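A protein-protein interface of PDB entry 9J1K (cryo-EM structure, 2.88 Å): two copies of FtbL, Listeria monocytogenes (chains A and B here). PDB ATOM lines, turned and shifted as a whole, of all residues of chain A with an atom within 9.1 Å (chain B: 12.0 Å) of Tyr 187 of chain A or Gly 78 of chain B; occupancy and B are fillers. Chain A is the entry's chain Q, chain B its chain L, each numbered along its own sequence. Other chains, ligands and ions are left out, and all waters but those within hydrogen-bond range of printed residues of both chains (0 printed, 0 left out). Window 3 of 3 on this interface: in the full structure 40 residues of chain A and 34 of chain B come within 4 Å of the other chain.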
ATOM      1  N   GLN A 184      18.253  -7.177 -13.121  1.00  0.00           N
ATOM      2  CA  GLN A 184      18.139  -7.653 -11.752  1.00  0.00           C
ATOM      3  C   GLN A 184      17.685  -9.104 -11.736  1.00  0.00           C
ATOM      4  O   GLN A 184      17.005  -9.572 -12.654  1.00  0.00           O
ATOM      5  CB  GLN A 184      17.167  -6.785 -10.941  1.00  0.00           C
ATOM      6  CG  GLN A 184      15.703  -7.002 -11.278  1.00  0.00           C
ATOM      7  CD  GLN A 184      14.829  -5.852 -10.829  1.00  0.00           C
ATOM      8  OE1 GLN A 184      13.861  -6.042 -10.093  1.00  0.00           O
ATOM      9  NE2 GLN A 184      15.164  -4.646 -11.271  1.00  0.00           N
ATOM     10  N   PHE A 185      18.076  -9.812 -10.680  1.00  0.00           N
ATOM     11  CA  PHE A 185      17.635 -11.177 -10.432  1.00  0.00           C
ATOM     12  C   PHE A 185      16.462 -11.143  -9.463  1.00  0.00           C
ATOM     13  O   PHE A 185      16.565 -10.558  -8.381  1.00  0.00           O
ATOM     14  CB  PHE A 185      18.765 -12.026  -9.851  1.00  0.00           C
ATOM     15  CG  PHE A 185      19.902 -12.259 -10.799  1.00  0.00           C
ATOM     16  CD1 PHE A 185      19.698 -12.905 -12.005  1.00  0.00           C
ATOM     17  CD2 PHE A 185      21.182 -11.843 -10.477  1.00  0.00           C
ATOM     18  CE1 PHE A 185      20.747 -13.123 -12.874  1.00  0.00           C
ATOM     19  CE2 PHE A 185      22.234 -12.060 -11.343  1.00  0.00           C
ATOM     20  CZ  PHE A 185      22.015 -12.701 -12.543  1.00  0.00           C
ATOM     21  N   ARG A 186      15.357 -11.772  -9.847  1.00  0.00           N
ATOM     22  CA  ARG A 186      14.149 -11.758  -9.038  1.00  0.00           C
ATOM     23  C   ARG A 186      13.676 -13.179  -8.781  1.00  0.00           C
ATOM     24  O   ARG A 186      13.687 -14.022  -9.684  1.00  0.00           O
ATOM     25  CB  ARG A 186      13.036 -10.951  -9.707  1.00  0.00           C
ATOM     26  CG  ARG A 186      13.138  -9.460  -9.458  1.00  0.00           C
ATOM     27  CD  ARG A 186      12.095  -9.006  -8.456  1.00  0.00           C
ATOM     28  NE  ARG A 186      12.006  -7.555  -8.377  1.00  0.00           N
ATOM     29  CZ  ARG A 186      11.507  -6.891  -7.344  1.00  0.00           C
ATOM     30  NH1 ARG A 186      11.041  -7.522  -6.279  1.00  0.00           N
ATOM     31  NH2 ARG A 186      11.475  -5.563  -7.380  1.00  0.00           N
ATOM     32  N   TYR A 187      13.267 -13.434  -7.544  1.00  0.00           N
ATOM     33  CA  TYR A 187      12.762 -14.746  -7.170  1.00  0.00           C
ATOM     34  C   TYR A 187      11.425 -15.009  -7.851  1.00  0.00           C
ATOM     35  O   TYR A 187      10.579 -14.116  -7.954  1.00  0.00           O
ATOM     36  CB  TYR A 187      12.633 -14.832  -5.649  1.00  0.00           C
ATOM     37  CG  TYR A 187      11.526 -15.721  -5.133  1.00  0.00           C
ATOM     38  CD1 TYR A 187      11.664 -17.101  -5.128  1.00  0.00           C
ATOM     39  CD2 TYR A 187      10.357 -15.178  -4.621  1.00  0.00           C
ATOM     40  CE1 TYR A 187      10.661 -17.916  -4.644  1.00  0.00           C
ATOM     41  CE2 TYR A 187       9.349 -15.984  -4.135  1.00  0.00           C
ATOM     42  CZ  TYR A 187       9.507 -17.352  -4.147  1.00  0.00           C
ATOM     43  OH  TYR A 187       8.503 -18.160  -3.667  1.00  0.00           O
ATOM     44  N   LEU A 188      11.263 -16.237  -8.351  1.00  0.00           N
ATOM     45  CA  LEU A 188      10.063 -16.701  -9.046  1.00  0.00           C
ATOM     46  C   LEU A 188       9.892 -16.072 -10.423  1.00  0.00           C
ATOM     47  O   LEU A 188       8.974 -16.445 -11.161  1.00  0.00           O
ATOM     48  CB  LEU A 188       8.804 -16.444  -8.211  1.00  0.00           C
ATOM     49  CG  LEU A 188       8.311 -17.574  -7.309  1.00  0.00           C
ATOM     50  CD1 LEU A 188       7.009 -17.176  -6.637  1.00  0.00           C
ATOM     51  CD2 LEU A 188       8.138 -18.855  -8.102  1.00  0.00           C
ATOM     52  N   TYR A 189      10.757 -15.128 -10.794  1.00  0.00           N
ATOM     53  CA  TYR A 189      10.647 -14.470 -12.091  1.00  0.00           C
ATOM     54  C   TYR A 189      11.617 -15.045 -13.116  1.00  0.00           C
ATOM     55  O   TYR A 189      11.198 -15.510 -14.180  1.00  0.00           O
ATOM     56  CB  TYR A 189      10.874 -12.960 -11.951  1.00  0.00           C
ATOM     57  CG  TYR A 189      10.775 -12.230 -13.269  1.00  0.00           C
ATOM     58  CD1 TYR A 189       9.555 -12.078 -13.909  1.00  0.00           C
ATOM     59  CD2 TYR A 189      11.906 -11.714 -13.884  1.00  0.00           C
ATOM     60  CE1 TYR A 189       9.461 -11.420 -15.117  1.00  0.00           C
ATOM     61  CE2 TYR A 189      11.822 -11.054 -15.093  1.00  0.00           C
ATOM     62  CZ  TYR A 189      10.597 -10.910 -15.704  1.00  0.00           C
ATOM     63  OH  TYR A 189      10.508 -10.253 -16.909  1.00  0.00           O
ATOM     64  N   ASN A 190      12.915 -15.021 -12.816  1.00  0.00           N
ATOM     65  CA  ASN A 190      13.926 -15.498 -13.748  1.00  0.00           C
ATOM     66  C   ASN A 190      14.967 -16.387 -13.082  1.00  0.00           C
ATOM     67  O   ASN A 190      16.003 -16.672 -13.695  1.00  0.00           O
ATOM     68  CB  ASN A 190      14.618 -14.318 -14.440  1.00  0.00           C
ATOM     69  CG  ASN A 190      15.018 -13.230 -13.468  1.00  0.00           C
ATOM     70  OD1 ASN A 190      14.872 -13.380 -12.256  1.00  0.00           O
ATOM     71  ND2 ASN A 190      15.525 -12.123 -13.996  1.00  0.00           N
ATOM     72  N   THR A 191      14.726 -16.832 -11.853  1.00  0.00           N
ATOM     73  CA  THR A 191      15.639 -17.718 -11.153  1.00  0.00           C
ATOM     74  C   THR A 191      14.882 -18.948 -10.676  1.00  0.00           C
ATOM     75  O   THR A 191      13.684 -18.888 -10.386  1.00  0.00           O
ATOM     76  CB  THR A 191      16.320 -17.012  -9.967  1.00  0.00           C
ATOM     77  OG1 THR A 191      17.400 -17.820  -9.483  1.00  0.00           O
ATOM     78  CG2 THR A 191      15.335 -16.762  -8.842  1.00  0.00           C
ATOM     79  N   GLU A 192      15.588 -20.077 -10.622  1.00  0.00           N
ATOM     80  CA  GLU A 192      14.987 -21.350 -10.249  1.00  0.00           C
ATOM     81  C   GLU A 192      15.557 -21.894  -8.945  1.00  0.00           C
ATOM     82  O   GLU A 192      14.802 -22.177  -8.011  1.00  0.00           O
ATOM     83  CB  GLU A 192      15.174 -22.369 -11.382  1.00  0.00           C
ATOM     84  CG  GLU A 192      15.114 -23.819 -10.934  1.00  0.00           C
ATOM     85  CD  GLU A 192      13.696 -24.294 -10.694  1.00  0.00           C
ATOM     86  OE1 GLU A 192      13.053 -24.761 -11.657  1.00  0.00           O
ATOM     87  OE2 GLU A 192      13.223 -24.198  -9.543  1.00  0.00           O
ATOM     88  N   GLU A 193      16.875 -22.050  -8.855  1.00  0.00           N
ATOM     89  CA  GLU A 193      17.513 -22.603  -7.669  1.00  0.00           C
ATOM     90  C   GLU A 193      18.588 -21.643  -7.187  1.00  0.00           C
ATOM     91  O   GLU A 193      19.462 -21.242  -7.962  1.00  0.00           O
ATOM     92  CB  GLU A 193      18.120 -23.980  -7.957  1.00  0.00           C
ATOM     93  CG  GLU A 193      19.275 -24.352  -7.044  1.00  0.00           C
ATOM     94  CD  GLU A 193      19.717 -25.791  -7.221  1.00  0.00           C
ATOM     95  OE1 GLU A 193      19.570 -26.325  -8.340  1.00  0.00           O
ATOM     96  OE2 GLU A 193      20.212 -26.387  -6.241  1.00  0.00           O
ATOM     97  N   VAL A 194      18.518 -21.276  -5.911  1.00  0.00           N
ATOM     98  CA  VAL A 194      19.482 -20.385  -5.283  1.00  0.00           C
ATOM     99  C   VAL A 194      20.118 -21.125  -4.117  1.00  0.00           C
ATOM    100  O   VAL A 194      19.409 -21.667  -3.262  1.00  0.00           O
ATOM    101  CB  VAL A 194      18.822 -19.078  -4.808  1.00  0.00           C
ATOM    102  CG1 VAL A 194      19.875 -18.084  -4.363  1.00  0.00           C
ATOM    103  CG2 VAL A 194      17.964 -18.488  -5.913  1.00  0.00           C
ATOM    104  N   ILE A 277      23.357 -19.088  -8.407  1.00  0.00           N
ATOM    105  CA  ILE A 277      22.025 -18.774  -8.905  1.00  0.00           C
ATOM    106  C   ILE A 277      21.822 -19.474 -10.240  1.00  0.00           C
ATOM    107  O   ILE A 277      22.689 -19.410 -11.120  1.00  0.00           O
ATOM    108  CB  ILE A 277      21.819 -17.254  -9.055  1.00  0.00           C
ATOM    109  CG1 ILE A 277      21.708 -16.595  -7.681  1.00  0.00           C
ATOM    110  CG2 ILE A 277      20.585 -16.956  -9.889  1.00  0.00           C
ATOM    111  CD1 ILE A 277      21.379 -15.123  -7.741  1.00  0.00           C
ATOM    112  N   ALA A 278      20.678 -20.142 -10.386  1.00  0.00           N
ATOM    113  CA  ALA A 278      20.259 -20.734 -11.651  1.00  0.00           C
ATOM    114  C   ALA A 278      19.321 -19.750 -12.339  1.00  0.00           C
ATOM    115  O   ALA A 278      18.190 -19.541 -11.889  1.00  0.00           O
ATOM    116  CB  ALA A 278      19.581 -22.083 -11.428  1.00  0.00           C
ATOM    117  N   TYR A 292      21.187  -6.699  -9.465  1.00  0.00           N
ATOM    118  CA  TYR A 292      20.483  -6.497  -8.207  1.00  0.00           C
ATOM    119  C   TYR A 292      19.724  -7.774  -7.877  1.00  0.00           C
ATOM    120  O   TYR A 292      18.891  -8.227  -8.670  1.00  0.00           O
ATOM    121  CB  TYR A 292      19.532  -5.304  -8.290  1.00  0.00           C
ATOM    122  CG  TYR A 292      19.252  -4.664  -6.952  1.00  0.00           C
ATOM    123  CD1 TYR A 292      20.122  -3.729  -6.414  1.00  0.00           C
ATOM    124  CD2 TYR A 292      18.120  -5.000  -6.224  1.00  0.00           C
ATOM    125  CE1 TYR A 292      19.873  -3.142  -5.190  1.00  0.00           C
ATOM    126  CE2 TYR A 292      17.862  -4.419  -5.000  1.00  0.00           C
ATOM    127  CZ  TYR A 292      18.740  -3.491  -4.487  1.00  0.00           C
ATOM    128  OH  TYR A 292      18.486  -2.910  -3.267  1.00  0.00           O
ATOM    129  N   PHE A 293      20.009  -8.350  -6.716  1.00  0.00           N
ATOM    130  CA  PHE A 293      19.418  -9.615  -6.303  1.00  0.00           C
ATOM    131  C   PHE A 293      18.353  -9.344  -5.251  1.00  0.00           C
ATOM    132  O   PHE A 293      18.640  -8.727  -4.215  1.00  0.00           O
ATOM    133  CB  PHE A 293      20.482 -10.567  -5.762  1.00  0.00           C
ATOM    134  CG  PHE A 293      19.967 -11.947  -5.478  1.00  0.00           C
ATOM    135  CD1 PHE A 293      19.007 -12.522  -6.292  1.00  0.00           C
ATOM    136  CD2 PHE A 293      20.444 -12.672  -4.400  1.00  0.00           C
ATOM    137  CE1 PHE A 293      18.531 -13.790  -6.036  1.00  0.00           C
ATOM    138  CE2 PHE A 293      19.972 -13.941  -4.139  1.00  0.00           C
ATOM    139  CZ  PHE A 293      19.014 -14.502  -4.958  1.00  0.00           C
ATOM    140  N   ILE A 294      17.132  -9.799  -5.527  1.00  0.00           N
ATOM    141  CA  ILE A 294      16.005  -9.701  -4.607  1.00  0.00           C
ATOM    142  C   ILE A 294      15.397 -11.090  -4.470  1.00  0.00           C
ATOM    143  O   ILE A 294      14.958 -11.680  -5.465  1.00  0.00           O
ATOM    144  CB  ILE A 294      14.945  -8.699  -5.091  1.00  0.00           C
ATOM    145  CG1 ILE A 294      15.537  -7.294  -5.189  1.00  0.00           C
ATOM    146  CG2 ILE A 294      13.744  -8.709  -4.161  1.00  0.00           C
ATOM    147  CD1 ILE A 294      14.893  -6.444  -6.256  1.00  0.00           C
ATOM    148  N   HIS A 295      15.370 -11.607  -3.245  1.00  0.00           N
ATOM    149  CA  HIS A 295      14.840 -12.939  -2.967  1.00  0.00           C
ATOM    150  C   HIS A 295      14.326 -12.915  -1.529  1.00  0.00           C
ATOM    151  O   HIS A 295      15.108 -13.079  -0.587  1.00  0.00           O
ATOM    152  CB  HIS A 295      15.908 -14.003  -3.168  1.00  0.00           C
ATOM    153  CG  HIS A 295      15.361 -15.376  -3.400  1.00  0.00           C
ATOM    154  ND1 HIS A 295      15.566 -16.069  -4.573  1.00  0.00           N
ATOM    155  CD2 HIS A 295      14.615 -16.182  -2.611  1.00  0.00           C
ATOM    156  CE1 HIS A 295      14.971 -17.247  -4.494  1.00  0.00           C
ATOM    157  NE2 HIS A 295      14.386 -17.340  -3.314  1.00  0.00           N
ATOM    158  N   GLU A 296      13.020 -12.699  -1.372  1.00  0.00           N
ATOM    159  CA  GLU A 296      12.450 -12.525  -0.036  1.00  0.00           C
ATOM    160  C   GLU A 296      12.582 -13.761   0.846  1.00  0.00           C
ATOM    161  O   GLU A 296      13.016 -13.615   2.003  1.00  0.00           O
ATOM    162  CB  GLU A 296      10.989 -12.076  -0.155  1.00  0.00           C
ATOM    163  CG  GLU A 296      10.785 -10.843  -1.022  1.00  0.00           C
ATOM    164  CD  GLU A 296      10.575 -11.185  -2.484  1.00  0.00           C
ATOM    165  OE1 GLU A 296      10.571 -12.387  -2.820  1.00  0.00           O
ATOM    166  OE2 GLU A 296      10.418 -10.250  -3.297  1.00  0.00           O
ATOM    167  N   PRO A 297      12.229 -14.976   0.404  1.00  0.00           N
ATOM    168  CA  PRO A 297      12.366 -16.131   1.311  1.00  0.00           C
ATOM    169  C   PRO A 297      13.789 -16.378   1.775  1.00  0.00           C
ATOM    170  O   PRO A 297      13.988 -16.863   2.895  1.00  0.00           O
ATOM    171  CB  PRO A 297      11.829 -17.305   0.476  1.00  0.00           C
ATOM    172  CG  PRO A 297      11.818 -16.828  -0.924  1.00  0.00           C
ATOM    173  CD  PRO A 297      11.582 -15.361  -0.861  1.00  0.00           C
ATOM    174  N   MET A 298      14.787 -16.062   0.955  1.00  0.00           N
ATOM    175  CA  MET A 298      16.180 -16.191   1.356  1.00  0.00           C
ATOM    176  C   MET A 298      16.712 -14.945   2.050  1.00  0.00           C
ATOM    177  O   MET A 298      17.878 -14.933   2.460  1.00  0.00           O
ATOM    178  CB  MET A 298      17.052 -16.517   0.140  1.00  0.00           C
ATOM    179  CG  MET A 298      16.701 -17.829  -0.538  1.00  0.00           C
ATOM    180  SD  MET A 298      17.559 -19.241   0.180  1.00  0.00           S
ATOM    181  CE  MET A 298      19.235 -18.919  -0.355  1.00  0.00           C
ATOM    182  N   GLY A 299      15.894 -13.907   2.195  1.00  0.00           N
ATOM    183  CA  GLY A 299      16.316 -12.692   2.865  1.00  0.00           C
ATOM    184  C   GLY A 299      17.433 -11.964   2.149  1.00  0.00           C
ATOM    185  O   GLY A 299      18.411 -11.545   2.775  1.00  0.00           O
ATOM    186  N   PHE A 300      17.302 -11.808   0.835  1.00  0.00           N
ATOM    187  CA  PHE A 300      18.317 -11.167   0.011  1.00  0.00           C
ATOM    188  C   PHE A 300      17.735  -9.923  -0.643  1.00  0.00           C
ATOM    189  O   PHE A 300      16.704  -9.999  -1.312  1.00  0.00           O
ATOM    190  CB  PHE A 300      18.831 -12.123  -1.066  1.00  0.00           C
ATOM    191  CG  PHE A 300      20.100 -12.830  -0.696  1.00  0.00           C
ATOM    192  CD1 PHE A 300      21.328 -12.230  -0.908  1.00  0.00           C
ATOM    193  CD2 PHE A 300      20.064 -14.099  -0.145  1.00  0.00           C
ATOM    194  CE1 PHE A 300      22.498 -12.880  -0.570  1.00  0.00           C
ATOM    195  CE2 PHE A 300      21.230 -14.753   0.195  1.00  0.00           C
ATOM    196  CZ  PHE A 300      22.448 -14.143  -0.019  1.00  0.00           C
ATOM    197  N   ASN B  42      13.491 -28.080   6.845  1.00  0.00           N
ATOM    198  CA  ASN B  42      12.630 -27.415   5.880  1.00  0.00           C
ATOM    199  C   ASN B  42      11.801 -26.348   6.581  1.00  0.00           C
ATOM    200  O   ASN B  42      11.268 -26.577   7.670  1.00  0.00           O
ATOM    201  CB  ASN B  42      11.709 -28.418   5.184  1.00  0.00           C
ATOM    202  CG  ASN B  42      12.314 -28.979   3.915  1.00  0.00           C
ATOM    203  OD1 ASN B  42      13.443 -29.467   3.915  1.00  0.00           O
ATOM    204  ND2 ASN B  42      11.563 -28.913   2.824  1.00  0.00           N
ATOM    205  N   LYS B  43      11.696 -25.181   5.952  1.00  0.00           N
ATOM    206  CA  LYS B  43      10.943 -24.069   6.521  1.00  0.00           C
ATOM    207  C   LYS B  43       9.454 -24.355   6.381  1.00  0.00           C
ATOM    208  O   LYS B  43       8.927 -24.414   5.266  1.00  0.00           O
ATOM    209  CB  LYS B  43      11.316 -22.761   5.832  1.00  0.00           C
ATOM    210  CG  LYS B  43      10.410 -21.597   6.189  1.00  0.00           C
ATOM    211  CD  LYS B  43      11.123 -20.269   6.011  1.00  0.00           C
ATOM    212  CE  LYS B  43      10.322 -19.128   6.611  1.00  0.00           C
ATOM    213  NZ  LYS B  43       8.951 -19.055   6.038  1.00  0.00           N
ATOM    214  N   THR B  44       8.775 -24.536   7.511  1.00  0.00           N
ATOM    215  CA  THR B  44       7.340 -24.776   7.550  1.00  0.00           C
ATOM    216  C   THR B  44       6.699 -23.783   8.510  1.00  0.00           C
ATOM    217  O   THR B  44       7.375 -22.952   9.121  1.00  0.00           O
ATOM    218  CB  THR B  44       7.023 -26.217   7.971  1.00  0.00           C
ATOM    219  OG1 THR B  44       7.526 -26.450   9.292  1.00  0.00           O
ATOM    220  CG2 THR B  44       7.656 -27.209   7.009  1.00  0.00           C
ATOM    221  N   PHE B  51      13.067 -20.065  12.033  1.00  0.00           N
ATOM    222  CA  PHE B  51      13.866 -20.600  10.937  1.00  0.00           C
ATOM    223  C   PHE B  51      14.996 -19.663  10.535  1.00  0.00           C
ATOM    224  O   PHE B  51      15.984 -20.115   9.948  1.00  0.00           O
ATOM    225  CB  PHE B  51      12.978 -20.892   9.727  1.00  0.00           C
ATOM    226  CG  PHE B  51      13.671 -21.661   8.639  1.00  0.00           C
ATOM    227  CD1 PHE B  51      13.747 -23.042   8.694  1.00  0.00           C
ATOM    228  CD2 PHE B  51      14.242 -21.007   7.562  1.00  0.00           C
ATOM    229  CE1 PHE B  51      14.381 -23.754   7.697  1.00  0.00           C
ATOM    230  CE2 PHE B  51      14.879 -21.714   6.562  1.00  0.00           C
ATOM    231  CZ  PHE B  51      14.947 -23.088   6.631  1.00  0.00           C
ATOM    232  N   PRO B  74      21.650 -22.888   3.070  1.00  0.00           N
ATOM    233  CA  PRO B  74      20.290 -22.541   2.647  1.00  0.00           C
ATOM    234  C   PRO B  74      20.105 -22.813   1.162  1.00  0.00           C
ATOM    235  O   PRO B  74      21.003 -22.575   0.351  1.00  0.00           O
ATOM    236  CB  PRO B  74      20.186 -21.046   2.965  1.00  0.00           C
ATOM    237  CG  PRO B  74      21.245 -20.792   3.981  1.00  0.00           C
ATOM    238  CD  PRO B  74      22.356 -21.739   3.661  1.00  0.00           C
ATOM    239  N   LYS B  75      18.927 -23.317   0.810  1.00  0.00           N
ATOM    240  CA  LYS B  75      18.626 -23.652  -0.573  1.00  0.00           C
ATOM    241  C   LYS B  75      17.157 -23.366  -0.837  1.00  0.00           C
ATOM    242  O   LYS B  75      16.306 -23.630   0.015  1.00  0.00           O
ATOM    243  CB  LYS B  75      18.953 -25.118  -0.874  1.00  0.00           C
ATOM    244  CG  LYS B  75      18.809 -25.503  -2.333  1.00  0.00           C
ATOM    245  CD  LYS B  75      19.027 -26.992  -2.529  1.00  0.00           C
ATOM    246  CE  LYS B  75      20.505 -27.320  -2.646  1.00  0.00           C
ATOM    247  NZ  LYS B  75      20.925 -27.487  -4.064  1.00  0.00           N
ATOM    248  N   SER B  76      16.867 -22.829  -2.019  1.00  0.00           N
ATOM    249  CA  SER B  76      15.510 -22.448  -2.396  1.00  0.00           C
ATOM    250  C   SER B  76      15.184 -23.072  -3.745  1.00  0.00           C
ATOM    251  O   SER B  76      15.757 -22.684  -4.767  1.00  0.00           O
ATOM    252  CB  SER B  76      15.361 -20.928  -2.452  1.00  0.00           C
ATOM    253  OG  SER B  76      14.202 -20.559  -3.179  1.00  0.00           O
ATOM    254  N   ILE B  77      14.271 -24.034  -3.745  1.00  0.00           N
ATOM    255  CA  ILE B  77      13.784 -24.664  -4.970  1.00  0.00           C
ATOM    256  C   ILE B  77      12.272 -24.472  -4.977  1.00  0.00           C
ATOM    257  O   ILE B  77      11.517 -25.283  -4.435  1.00  0.00           O
ATOM    258  CB  ILE B  77      14.163 -26.143  -5.061  1.00  0.00           C
ATOM    259  CG1 ILE B  77      15.659 -26.328  -4.810  1.00  0.00           C
ATOM    260  CG2 ILE B  77      13.778 -26.706  -6.419  1.00  0.00           C
ATOM    261  CD1 ILE B  77      16.057 -27.761  -4.551  1.00  0.00           C
ATOM    262  N   GLY B  78      11.819 -23.389  -5.601  1.00  0.00           N
ATOM    263  CA  GLY B  78      10.403 -23.088  -5.656  1.00  0.00           C
ATOM    264  C   GLY B  78       9.850 -22.550  -4.353  1.00  0.00           C
ATOM    265  O   GLY B  78      10.211 -21.451  -3.924  1.00  0.00           O
ATOM    266  N   GLY B  79       8.971 -23.318  -3.715  1.00  0.00           N
ATOM    267  CA  GLY B  79       8.327 -22.871  -2.496  1.00  0.00           C
ATOM    268  C   GLY B  79       8.921 -23.445  -1.228  1.00  0.00           C
ATOM    269  O   GLY B  79       8.484 -23.104  -0.125  1.00  0.00           O
ATOM    270  N   THR B  80       9.917 -24.314  -1.365  1.00  0.00           N
ATOM    271  CA  THR B  80      10.544 -24.976  -0.231  1.00  0.00           C
ATOM    272  C   THR B  80      11.927 -24.387   0.006  1.00  0.00           C
ATOM    273  O   THR B  80      12.747 -24.327  -0.916  1.00  0.00           O
ATOM    274  CB  THR B  80      10.650 -26.485  -0.462  1.00  0.00           C
ATOM    275  OG1 THR B  80      11.979 -26.811  -0.887  1.00  0.00           O
ATOM    276  CG2 THR B  80       9.659 -26.933  -1.525  1.00  0.00           C
ATOM    277  N   ILE B  81      12.177 -23.955   1.238  1.00  0.00           N
ATOM    278  CA  ILE B  81      13.482 -23.457   1.657  1.00  0.00           C
ATOM    279  C   ILE B  81      14.057 -24.460   2.644  1.00  0.00           C
ATOM    280  O   ILE B  81      13.438 -24.751   3.675  1.00  0.00           O
ATOM    281  CB  ILE B  81      13.384 -22.058   2.282  1.00  0.00           C
ATOM    282  CG1 ILE B  81      12.326 -21.225   1.562  1.00  0.00           C
ATOM    283  CG2 ILE B  81      14.734 -21.362   2.240  1.00  0.00           C
ATOM    284  CD1 ILE B  81      12.693 -20.870   0.139  1.00  0.00           C
ATOM    285  N   SER B  82      15.237 -24.988   2.333  1.00  0.00           N
ATOM    286  CA  SER B  82      15.855 -26.029   3.139  1.00  0.00           C
ATOM    287  C   SER B  82      17.269 -25.619   3.520  1.00  0.00           C
ATOM    288  O   SER B  82      17.999 -25.039   2.712  1.00  0.00           O
ATOM    289  CB  SER B  82      15.884 -27.364   2.391  1.00  0.00           C
ATOM    290  OG  SER B  82      16.647 -27.265   1.202  1.00  0.00           O
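O of Glu 192 of chain A lies close to O of Ser 76 of chain B, 3.4 Å away. N of Ser 76 of chain B sits at hydrogen-bond distance from O of Val 194 of chain A, at 3.1 Å. The side-chain amino group (NZ) of Lys 75 of chain B is in salt-bridge range of the side-chain carboxylate (OE2) of Glu 193 of chain A (2.5 Å). The side-chain hydroxyl (OG) of Ser 76 of chain B lies within hydrogen-bond range of a ring nitrogen (NE2) of His 295 of chain A, 3.2 Å away.
O of Ile 81 of chain B lies within hydrogen-bond range of N of Lys 43 of chain B (2.9 Å). The backbone NH (N) of Lys 75 of chain B sits at hydrogen-bond distance from the backbone carbonyl oxygen (O) of Ser 82 of chain B (2.7 Å). N of Tyr 187 of chain A lies within hydrogen-bond range of O of Ile 294 of chain A (3.2 Å). N of His 295 of chain A lies within hydrogen-bond range of O of Phe 300 of chain A (2.8 Å). The backbone carbonyl oxygen (O) of Ala 278 of chain A is in hydrogen-bond range of the backbone NH (N) of Glu 192 of chain A, at 2.9 Å. The backbone carbonyl oxygen (O) of Glu 193 of chain A sits at hydrogen-bond distance from the backbone NH (N) of Ala 278 of chain A.
O of Gly 78 of chain B touches CE1 of Tyr 187 of chain A, at 3.6 Å. Glu 193 of chain A touches Ser 76 of chain B. Val 194 of chain A touches Lys 75 of chain B. CB of Pro 297 of chain A touches CD1 of Ile 81 of chain B (3.7 Å). Met 298 of chain A touches Ser 76 of chain B.
Tyr 187 of chain A touches just one residue of chain B: Gly 78 (3.6 Å). Leu 188 of chain A touches none of the printed residues of chain B. No residue of chain B comes within 4 Å of Asn 190 of chain A. No residue of chain B comes within 4 Å of Thr 191 of chain A. Of the printed residues of chain B, Val 194 of chain A touches Lys 75 and Ser 76. No residue of chain B comes within 4 Å of Ile 294 of chain A. His 295 of chain A touches just one residue of chain B: Ser 76 (3.2 Å). No residue of chain B comes within 4 Å of Glu 296 of chain A. Of the printed residues of chain B, Pro 297 of chain A touches Ile 81. Of the printed residues of chain B, Met 298 of chain A touches Ser 76. Gly 299 of chain A touches none of the printed residues of chain B. Thr 44 of chain B touches none of the printed residues of chain A. Gly 78 of chain B touches just one residue of chain A: Tyr 187 (3.6 Å). No residue of chain A comes within 4 Å of Gly 79 of chain B. Of the printed residues of chain A, Ile 81 of chain B touches Pro 297 (3.7 Å). The nearest residue of chain B that does not touch Tyr 187 of chain A is Ser 76 of chain B (4.7 Å). The nearest residue of chain A that does not touch Gly 78 of chain B is Glu 192 of chain A (4.02 Å).
Of the 22 printed residues of chain A, 7 touch a printed residue of chain B. Hydrophobic or aromatic side chains of chain A that line the printed part of chain B: Tyr 187, His 295, Pro 297 and Met 298. Of the 13 printed residues of chain B, 4 touch a printed residue of chain A. Among the printed residues, Asp or Glu carboxylates within 4 Å of a Lys or Arg side-chain nitrogen of the other chain: Glu 193 of chain A with Lys 75 of chain B (2.5 Å).
No position is printed for both chains.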
